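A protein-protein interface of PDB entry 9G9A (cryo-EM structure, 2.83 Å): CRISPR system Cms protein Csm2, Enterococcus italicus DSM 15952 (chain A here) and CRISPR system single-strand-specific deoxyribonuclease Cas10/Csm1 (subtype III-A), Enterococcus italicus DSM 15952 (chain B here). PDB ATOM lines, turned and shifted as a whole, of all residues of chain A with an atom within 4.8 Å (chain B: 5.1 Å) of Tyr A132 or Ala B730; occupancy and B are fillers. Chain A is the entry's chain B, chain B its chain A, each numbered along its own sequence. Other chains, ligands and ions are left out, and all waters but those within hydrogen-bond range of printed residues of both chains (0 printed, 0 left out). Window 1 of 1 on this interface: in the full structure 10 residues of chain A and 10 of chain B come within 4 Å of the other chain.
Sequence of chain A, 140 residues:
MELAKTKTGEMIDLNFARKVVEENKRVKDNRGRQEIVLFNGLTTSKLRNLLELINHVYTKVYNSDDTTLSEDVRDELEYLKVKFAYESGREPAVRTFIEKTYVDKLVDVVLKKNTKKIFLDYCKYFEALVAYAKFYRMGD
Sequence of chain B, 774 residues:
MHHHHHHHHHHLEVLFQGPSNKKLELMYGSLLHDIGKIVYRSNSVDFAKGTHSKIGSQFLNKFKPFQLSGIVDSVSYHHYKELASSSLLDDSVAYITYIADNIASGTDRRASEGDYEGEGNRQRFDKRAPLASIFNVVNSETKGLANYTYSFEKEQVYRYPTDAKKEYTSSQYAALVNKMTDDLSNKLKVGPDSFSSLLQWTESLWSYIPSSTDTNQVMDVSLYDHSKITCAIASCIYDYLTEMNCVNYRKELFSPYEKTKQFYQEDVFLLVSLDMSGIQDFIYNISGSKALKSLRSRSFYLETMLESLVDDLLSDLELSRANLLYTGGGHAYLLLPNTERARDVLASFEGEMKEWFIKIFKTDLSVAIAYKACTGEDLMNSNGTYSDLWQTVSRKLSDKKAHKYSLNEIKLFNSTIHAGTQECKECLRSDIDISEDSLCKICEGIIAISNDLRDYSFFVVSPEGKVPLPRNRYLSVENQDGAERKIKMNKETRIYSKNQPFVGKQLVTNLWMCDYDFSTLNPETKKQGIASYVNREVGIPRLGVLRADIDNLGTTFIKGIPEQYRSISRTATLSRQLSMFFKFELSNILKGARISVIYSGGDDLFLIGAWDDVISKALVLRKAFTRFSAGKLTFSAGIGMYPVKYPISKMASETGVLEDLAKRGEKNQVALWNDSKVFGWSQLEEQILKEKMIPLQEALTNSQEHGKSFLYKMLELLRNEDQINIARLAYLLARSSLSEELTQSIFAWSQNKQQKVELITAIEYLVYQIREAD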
ATOM      1  N   ALA A  17      16.058   9.673  -6.429  1.00  0.00           N
ATOM      2  CA  ALA A  17      16.937  10.828  -6.271  1.00  0.00           C
ATOM      3  C   ALA A  17      16.170  12.033  -5.741  1.00  0.00           C
ATOM      4  O   ALA A  17      16.646  12.753  -4.854  1.00  0.00           O
ATOM      5  CB  ALA A  17      17.608  11.157  -7.605  1.00  0.00           C
ATOM      6  N   ARG A  18      14.969  12.263  -6.276  1.00  0.00           N
ATOM      7  CA  ARG A  18      14.154  13.381  -5.817  1.00  0.00           C
ATOM      8  C   ARG A  18      13.813  13.240  -4.339  1.00  0.00           C
ATOM      9  O   ARG A  18      13.902  14.210  -3.578  1.00  0.00           O
ATOM     10  CB  ARG A  18      12.881  13.476  -6.658  1.00  0.00           C
ATOM     11  CG  ARG A  18      12.166  14.812  -6.570  1.00  0.00           C
ATOM     12  CD  ARG A  18      10.950  14.833  -7.481  1.00  0.00           C
ATOM     13  NE  ARG A  18      10.433  16.180  -7.683  1.00  0.00           N
ATOM     14  CZ  ARG A  18       9.496  16.744  -6.934  1.00  0.00           C
ATOM     15  NH1 ARG A  18       8.950  16.105  -5.913  1.00  0.00           N
ATOM     16  NH2 ARG A  18       9.096  17.981  -7.216  1.00  0.00           N
ATOM     17  N   VAL A  21      16.910  13.778  -2.104  1.00  0.00           N
ATOM     18  CA  VAL A  21      17.360  15.165  -2.033  1.00  0.00           C
ATOM     19  C   VAL A  21      16.338  16.028  -1.300  1.00  0.00           C
ATOM     20  O   VAL A  21      16.700  17.039  -0.684  1.00  0.00           O
ATOM     21  CB  VAL A  21      17.671  15.712  -3.439  1.00  0.00           C
ATOM     22  CG1 VAL A  21      16.399  15.974  -4.217  1.00  0.00           C
ATOM     23  CG2 VAL A  21      18.515  16.974  -3.342  1.00  0.00           C
ATOM     24  N   ALA A 128      20.649  12.958 -12.195  1.00  0.00           N
ATOM     25  CA  ALA A 128      19.380  13.337 -11.587  1.00  0.00           C
ATOM     26  C   ALA A 128      19.588  13.860 -10.173  1.00  0.00           C
ATOM     27  O   ALA A 128      18.935  14.823  -9.758  1.00  0.00           O
ATOM     28  CB  ALA A 128      18.420  12.148 -11.588  1.00  0.00           C
ATOM     29  N   LEU A 129      20.500  13.239  -9.421  1.00  0.00           N
ATOM     30  CA  LEU A 129      20.795  13.704  -8.070  1.00  0.00           C
ATOM     31  C   LEU A 129      21.298  15.142  -8.084  1.00  0.00           C
ATOM     32  O   LEU A 129      20.798  15.992  -7.340  1.00  0.00           O
ATOM     33  CB  LEU A 129      21.826  12.783  -7.415  1.00  0.00           C
ATOM     34  CG  LEU A 129      21.620  12.388  -5.948  1.00  0.00           C
ATOM     35  CD1 LEU A 129      21.022  13.525  -5.129  1.00  0.00           C
ATOM     36  CD2 LEU A 129      20.765  11.138  -5.843  1.00  0.00           C
ATOM     37  N   VAL A 130      22.289  15.435  -8.930  1.00  0.00           N
ATOM     38  CA  VAL A 130      22.851  16.784  -8.947  1.00  0.00           C
ATOM     39  C   VAL A 130      21.842  17.786  -9.503  1.00  0.00           C
ATOM     40  O   VAL A 130      21.756  18.929  -9.029  1.00  0.00           O
ATOM     41  CB  VAL A 130      24.188  16.810  -9.717  1.00  0.00           C
ATOM     42  CG1 VAL A 130      24.004  16.394 -11.161  1.00  0.00           C
ATOM     43  CG2 VAL A 130      24.827  18.189  -9.630  1.00  0.00           C
ATOM     44  N   ALA A 131      21.047  17.377 -10.496  1.00  0.00           N
ATOM     45  CA  ALA A 131      20.031  18.263 -11.053  1.00  0.00           C
ATOM     46  C   ALA A 131      18.985  18.625 -10.007  1.00  0.00           C
ATOM     47  O   ALA A 131      18.604  19.792  -9.873  1.00  0.00           O
ATOM     48  CB  ALA A 131      19.374  17.606 -12.267  1.00  0.00           C
ATOM     49  N   TYR A 132      18.506  17.632  -9.254  1.00  0.00           N
ATOM     50  CA  TYR A 132      17.537  17.907  -8.200  1.00  0.00           C
ATOM     51  C   TYR A 132      18.157  18.703  -7.060  1.00  0.00           C
ATOM     52  O   TYR A 132      17.472  19.523  -6.438  1.00  0.00           O
ATOM     53  CB  TYR A 132      16.945  16.599  -7.679  1.00  0.00           C
ATOM     54  CG  TYR A 132      15.933  15.969  -8.608  1.00  0.00           C
ATOM     55  CD1 TYR A 132      15.011  16.748  -9.293  1.00  0.00           C
ATOM     56  CD2 TYR A 132      15.903  14.596  -8.805  1.00  0.00           C
ATOM     57  CE1 TYR A 132      14.086  16.177 -10.144  1.00  0.00           C
ATOM     58  CE2 TYR A 132      14.982  14.016  -9.655  1.00  0.00           C
ATOM     59  CZ  TYR A 132      14.076  14.811 -10.321  1.00  0.00           C
ATOM     60  OH  TYR A 132      13.156  14.235 -11.167  1.00  0.00           O
ATOM     61  N   ALA A 133      19.440  18.480  -6.768  1.00  0.00           N
ATOM     62  CA  ALA A 133      20.111  19.273  -5.745  1.00  0.00           C
ATOM     63  C   ALA A 133      20.170  20.740  -6.144  1.00  0.00           C
ATOM     64  O   ALA A 133      19.959  21.627  -5.311  1.00  0.00           O
ATOM     65  CB  ALA A 133      21.515  18.725  -5.492  1.00  0.00           C
ATOM     66  N   LYS A 134      20.456  21.017  -7.418  1.00  0.00           N
ATOM     67  CA  LYS A 134      20.440  22.402  -7.881  1.00  0.00           C
ATOM     68  C   LYS A 134      19.021  22.948  -7.979  1.00  0.00           C
ATOM     69  O   LYS A 134      18.814  24.160  -7.837  1.00  0.00           O
ATOM     70  CB  LYS A 134      21.145  22.520  -9.232  1.00  0.00           C
ATOM     71  CG  LYS A 134      22.660  22.464  -9.149  1.00  0.00           C
ATOM     72  CD  LYS A 134      23.207  23.550  -8.234  1.00  0.00           C
ATOM     73  CE  LYS A 134      22.769  24.939  -8.676  1.00  0.00           C
ATOM     74  NZ  LYS A 134      23.075  25.189 -10.107  1.00  0.00           N
ATOM     75  N   PHE A 135      18.038  22.078  -8.223  1.00  0.00           N
ATOM     76  CA  PHE A 135      16.658  22.524  -8.372  1.00  0.00           C
ATOM     77  C   PHE A 135      16.085  23.046  -7.062  1.00  0.00           C
ATOM     78  O   PHE A 135      15.293  23.996  -7.066  1.00  0.00           O
ATOM     79  CB  PHE A 135      15.802  21.377  -8.912  1.00  0.00           C
ATOM     80  CG  PHE A 135      14.355  21.732  -9.099  1.00  0.00           C
ATOM     81  CD1 PHE A 135      13.967  22.599 -10.105  1.00  0.00           C
ATOM     82  CD2 PHE A 135      13.382  21.184  -8.279  1.00  0.00           C
ATOM     83  CE1 PHE A 135      12.636  22.922 -10.285  1.00  0.00           C
ATOM     84  CE2 PHE A 135      12.049  21.504  -8.454  1.00  0.00           C
ATOM     85  CZ  PHE A 135      11.676  22.374  -9.458  1.00  0.00           C
ATOM     86  N   TYR A 136      16.463  22.446  -5.937  1.00  0.00           N
ATOM     87  CA  TYR A 136      15.944  22.844  -4.637  1.00  0.00           C
ATOM     88  C   TYR A 136      16.781  23.921  -3.960  1.00  0.00           C
ATOM     89  O   TYR A 136      16.478  24.294  -2.823  1.00  0.00           O
ATOM     90  CB  TYR A 136      15.829  21.627  -3.715  1.00  0.00           C
ATOM     91  CG  TYR A 136      14.712  20.681  -4.090  1.00  0.00           C
ATOM     92  CD1 TYR A 136      13.382  21.050  -3.938  1.00  0.00           C
ATOM     93  CD2 TYR A 136      14.985  19.416  -4.588  1.00  0.00           C
ATOM     94  CE1 TYR A 136      12.357  20.188  -4.281  1.00  0.00           C
ATOM     95  CE2 TYR A 136      13.968  18.548  -4.932  1.00  0.00           C
ATOM     96  CZ  TYR A 136      12.658  18.937  -4.776  1.00  0.00           C
ATOM     97  OH  TYR A 136      11.646  18.071  -5.117  1.00  0.00           O
ATOM     98  N   GLN B 723      12.066  10.242 -17.720  1.00  0.00           N
ATOM     99  CA  GLN B 723      12.348  10.850 -16.422  1.00  0.00           C
ATOM    100  C   GLN B 723      13.694  11.562 -16.410  1.00  0.00           C
ATOM    101  O   GLN B 723      13.883  12.525 -15.654  1.00  0.00           O
ATOM    102  CB  GLN B 723      12.294   9.790 -15.322  1.00  0.00           C
ATOM    103  CG  GLN B 723      10.904   9.221 -15.086  1.00  0.00           C
ATOM    104  CD  GLN B 723      10.848   8.297 -13.887  1.00  0.00           C
ATOM    105  OE1 GLN B 723      11.823   7.621 -13.561  1.00  0.00           O
ATOM    106  NE2 GLN B 723       9.701   8.269 -13.217  1.00  0.00           N
ATOM    107  N   ASN B 725      14.710  13.353 -18.842  1.00  0.00           N
ATOM    108  CA  ASN B 725      14.322  14.676 -19.312  1.00  0.00           C
ATOM    109  C   ASN B 725      13.642  15.481 -18.212  1.00  0.00           C
ATOM    110  O   ASN B 725      13.759  16.707 -18.190  1.00  0.00           O
ATOM    111  CB  ASN B 725      13.413  14.556 -20.532  1.00  0.00           C
ATOM    112  CG  ASN B 725      14.122  13.949 -21.723  1.00  0.00           C
ATOM    113  OD1 ASN B 725      14.138  12.731 -21.896  1.00  0.00           O
ATOM    114  ND2 ASN B 725      14.715  14.799 -22.554  1.00  0.00           N
ATOM    115  N   ILE B 726      12.945  14.816 -17.288  1.00  0.00           N
ATOM    116  CA  ILE B 726      12.364  15.525 -16.149  1.00  0.00           C
ATOM    117  C   ILE B 726      13.462  16.115 -15.274  1.00  0.00           C
ATOM    118  O   ILE B 726      13.388  17.276 -14.848  1.00  0.00           O
ATOM    119  CB  ILE B 726      11.443  14.587 -15.348  1.00  0.00           C
ATOM    120  CG1 ILE B 726      10.369  13.988 -16.257  1.00  0.00           C
ATOM    121  CG2 ILE B 726      10.810  15.329 -14.184  1.00  0.00           C
ATOM    122  CD1 ILE B 726       9.461  15.017 -16.893  1.00  0.00           C
ATOM    123  N   ALA B 727      14.504  15.326 -14.993  1.00  0.00           N
ATOM    124  CA  ALA B 727      15.624  15.836 -14.207  1.00  0.00           C
ATOM    125  C   ALA B 727      16.350  16.959 -14.942  1.00  0.00           C
ATOM    126  O   ALA B 727      16.770  17.949 -14.328  1.00  0.00           O
ATOM    127  CB  ALA B 727      16.589  14.702 -13.869  1.00  0.00           C
ATOM    128  N   ARG B 728      16.513  16.817 -16.259  1.00  0.00           N
ATOM    129  CA  ARG B 728      17.153  17.870 -17.041  1.00  0.00           C
ATOM    130  C   ARG B 728      16.324  19.149 -17.030  1.00  0.00           C
ATOM    131  O   ARG B 728      16.879  20.251 -16.967  1.00  0.00           O
ATOM    132  CB  ARG B 728      17.391  17.385 -18.470  1.00  0.00           C
ATOM    133  CG  ARG B 728      18.452  16.305 -18.570  1.00  0.00           C
ATOM    134  CD  ARG B 728      18.357  15.537 -19.874  1.00  0.00           C
ATOM    135  NE  ARG B 728      19.317  14.441 -19.919  1.00  0.00           N
ATOM    136  CZ  ARG B 728      19.373  13.533 -20.884  1.00  0.00           C
ATOM    137  NH1 ARG B 728      18.530  13.554 -21.903  1.00  0.00           N
ATOM    138  NH2 ARG B 728      20.296  12.577 -20.823  1.00  0.00           N
ATOM    139  N   LEU B 729      14.997  19.024 -17.091  1.00  0.00           N
ATOM    140  CA  LEU B 729      14.131  20.193 -16.988  1.00  0.00           C
ATOM    141  C   LEU B 729      14.242  20.841 -15.616  1.00  0.00           C
ATOM    142  O   LEU B 729      14.230  22.071 -15.504  1.00  0.00           O
ATOM    143  CB  LEU B 729      12.684  19.802 -17.283  1.00  0.00           C
ATOM    144  CG  LEU B 729      11.666  20.944 -17.244  1.00  0.00           C
ATOM    145  CD1 LEU B 729      12.012  22.010 -18.270  1.00  0.00           C
ATOM    146  CD2 LEU B 729      10.266  20.413 -17.472  1.00  0.00           C
ATOM    147  N   ALA B 730      14.342  20.030 -14.560  1.00  0.00           N
ATOM    148  CA  ALA B 730      14.554  20.583 -13.226  1.00  0.00           C
ATOM    149  C   ALA B 730      15.860  21.368 -13.163  1.00  0.00           C
ATOM    150  O   ALA B 730      15.913  22.472 -12.607  1.00  0.00           O
ATOM    151  CB  ALA B 730      14.547  19.462 -12.186  1.00  0.00           C
ATOM    152  N   TYR B 731      16.925  20.814 -13.746  1.00  0.00           N
ATOM    153  CA  TYR B 731      18.204  21.520 -13.766  1.00  0.00           C
ATOM    154  C   TYR B 731      18.110  22.815 -14.565  1.00  0.00           C
ATOM    155  O   TYR B 731      18.659  23.848 -14.158  1.00  0.00           O
ATOM    156  CB  TYR B 731      19.293  20.614 -14.338  1.00  0.00           C
ATOM    157  CG  TYR B 731      20.666  21.246 -14.362  1.00  0.00           C
ATOM    158  CD1 TYR B 731      21.441  21.313 -13.212  1.00  0.00           C
ATOM    159  CD2 TYR B 731      21.188  21.776 -15.534  1.00  0.00           C
ATOM    160  CE1 TYR B 731      22.696  21.891 -13.229  1.00  0.00           C
ATOM    161  CE2 TYR B 731      22.442  22.355 -15.562  1.00  0.00           C
ATOM    162  CZ  TYR B 731      23.192  22.410 -14.406  1.00  0.00           C
ATOM    163  OH  TYR B 731      24.441  22.986 -14.431  1.00  0.00           O
ATOM    164  N   LEU B 732      17.419  22.780 -15.706  1.00  0.00           N
ATOM    165  CA  LEU B 732      17.264  23.976 -16.528  1.00  0.00           C
ATOM    166  C   LEU B 732      16.492  25.056 -15.782  1.00  0.00           C
ATOM    167  O   LEU B 732      16.842  26.240 -15.843  1.00  0.00           O
ATOM    168  CB  LEU B 732      16.565  23.620 -17.841  1.00  0.00           C
ATOM    169  CG  LEU B 732      16.388  24.760 -18.845  1.00  0.00           C
ATOM    170  CD1 LEU B 732      17.739  25.309 -19.272  1.00  0.00           C
ATOM    171  CD2 LEU B 732      15.592  24.294 -20.052  1.00  0.00           C
ATOM    172  N   LEU B 733      15.431  24.664 -15.074  1.00  0.00           N
ATOM    173  CA  LEU B 733      14.688  25.625 -14.264  1.00  0.00           C
ATOM    174  C   LEU B 733      15.559  26.184 -13.147  1.00  0.00           C
ATOM    175  O   LEU B 733      15.442  27.362 -12.790  1.00  0.00           O
ATOM    176  CB  LEU B 733      13.427  24.975 -13.697  1.00  0.00           C
ATOM    177  CG  LEU B 733      12.367  24.570 -14.723  1.00  0.00           C
ATOM    178  CD1 LEU B 733      11.130  24.032 -14.029  1.00  0.00           C
ATOM    179  CD2 LEU B 733      12.017  25.738 -15.628  1.00  0.00           C
ATOM    180  N   ALA B 734      16.434  25.351 -12.581  1.00  0.00           N
ATOM    181  CA  ALA B 734      17.371  25.834 -11.572  1.00  0.00           C
ATOM    182  C   ALA B 734      18.322  26.872 -12.157  1.00  0.00           C
ATOM    183  O   ALA B 734      18.664  27.859 -11.498  1.00  0.00           O
ATOM    184  CB  ALA B 734      18.150  24.659 -10.981  1.00  0.00           C
ATOM    185  N   PHE B 747       7.577  23.162 -12.962  1.00  0.00           N
ATOM    186  CA  PHE B 747       7.881  21.754 -12.732  1.00  0.00           C
ATOM    187  C   PHE B 747       6.618  20.963 -12.414  1.00  0.00           C
ATOM    188  O   PHE B 747       6.429  19.851 -12.921  1.00  0.00           O
ATOM    189  CB  PHE B 747       8.909  21.622 -11.608  1.00  0.00           C
ATOM    190  CG  PHE B 747       9.625  20.302 -11.592  1.00  0.00           C
ATOM    191  CD1 PHE B 747      10.372  19.891 -12.684  1.00  0.00           C
ATOM    192  CD2 PHE B 747       9.563  19.481 -10.480  1.00  0.00           C
ATOM    193  CE1 PHE B 747      11.034  18.678 -12.672  1.00  0.00           C
ATOM    194  CE2 PHE B 747      10.225  18.268 -10.462  1.00  0.00           C
ATOM    195  CZ  PHE B 747      10.961  17.868 -11.559  1.00  0.00           C
ATOM    196  N   GLN B 751       5.080  17.865 -14.578  1.00  0.00           N
ATOM    197  CA  GLN B 751       4.861  16.544 -13.997  1.00  0.00           C
ATOM    198  C   GLN B 751       3.450  16.036 -14.270  1.00  0.00           C
ATOM    199  O   GLN B 751       3.257  14.855 -14.581  1.00  0.00           O
ATOM    200  CB  GLN B 751       5.134  16.578 -12.492  1.00  0.00           C
ATOM    201  CG  GLN B 751       6.590  16.809 -12.113  1.00  0.00           C
ATOM    202  CD  GLN B 751       7.445  15.563 -12.246  1.00  0.00           C
ATOM    203  OE1 GLN B 751       7.046  14.581 -12.872  1.00  0.00           O
ATOM    204  NE2 GLN B 751       8.629  15.597 -11.649  1.00  0.00           N
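The side-chain hydroxyl (OH) of Tyr A136 sits close to the guanidinium group (NH2) of Arg A18, at 3.3 Å.
NH2 of Arg A18 touches CE2 of Phe B747, 3.4 Å away.
CB of Ala A131 touches O of Ala B727 (3.3 Å).
Ala A131 touches Tyr B731.
Tyr A132 touches Ile B726 (OH to CG2, 3.98 Å).
Tyr A132 touches Ala B730 (CE1 to CB, 3.9 Å).
CE1 of Tyr A132 touches CZ of Phe B747, 3.8 Å away.
Ala B734 touches Lys A134 (CB to O, 3.3 Å).
O of Ala B730 touches CD1 of Phe A135 (3.2 Å).
Ala B734 touches Phe A135 (CB to CA, 3.7 Å).
Phe A135 touches Phe B747 (CZ to CB, 3.6 Å).
Of the printed residues of chain B, Arg A18 touches Phe B747.
Tyr A132 touches three residues of chain B.
Of the printed residues of chain A, Ile B726 touches Tyr A132 (3.98 Å).
Of the printed residues of chain A, Ala B727 touches Ala A128 (3.9 Å) and Ala A131 (3.3 Å).
Of chain A, only Tyr A132 (3.9 Å) and Phe A135 (3.2 Å) come within 4 Å of Ala B730.
Of the printed residues of chain A, Tyr B731 touches Ala A131.
Of the printed residues of chain A, Phe B747 touches Arg A18, Tyr A132 and Phe A135.
The nearest residue of chain B that does not touch Tyr A132 is Ala B727 (4.2 Å).
The nearest residue of chain A that does not touch Ala B730 is Ala A131 (4.6 Å).
Hydrophobic or aromatic side chains of chain B that line the printed part of chain A: Ile B726, Ala B727, Ala B730, Tyr B731, Ala B734 and Phe B747.
Of the 12 printed residues of chain A, 6 touch a printed residue of chain B.
Printed residues of chain A that touch a printed residue of chain B: Arg A18, Ala A128, Ala A131, Tyr A132, Lys A134 and Phe A135.
Among the printed residues, 11 pairs touch across the chains.
Among the printed residues, no Asp or Glu carboxylate lies within 4 Å of a Lys or Arg side-chain nitrogen of the other chain.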
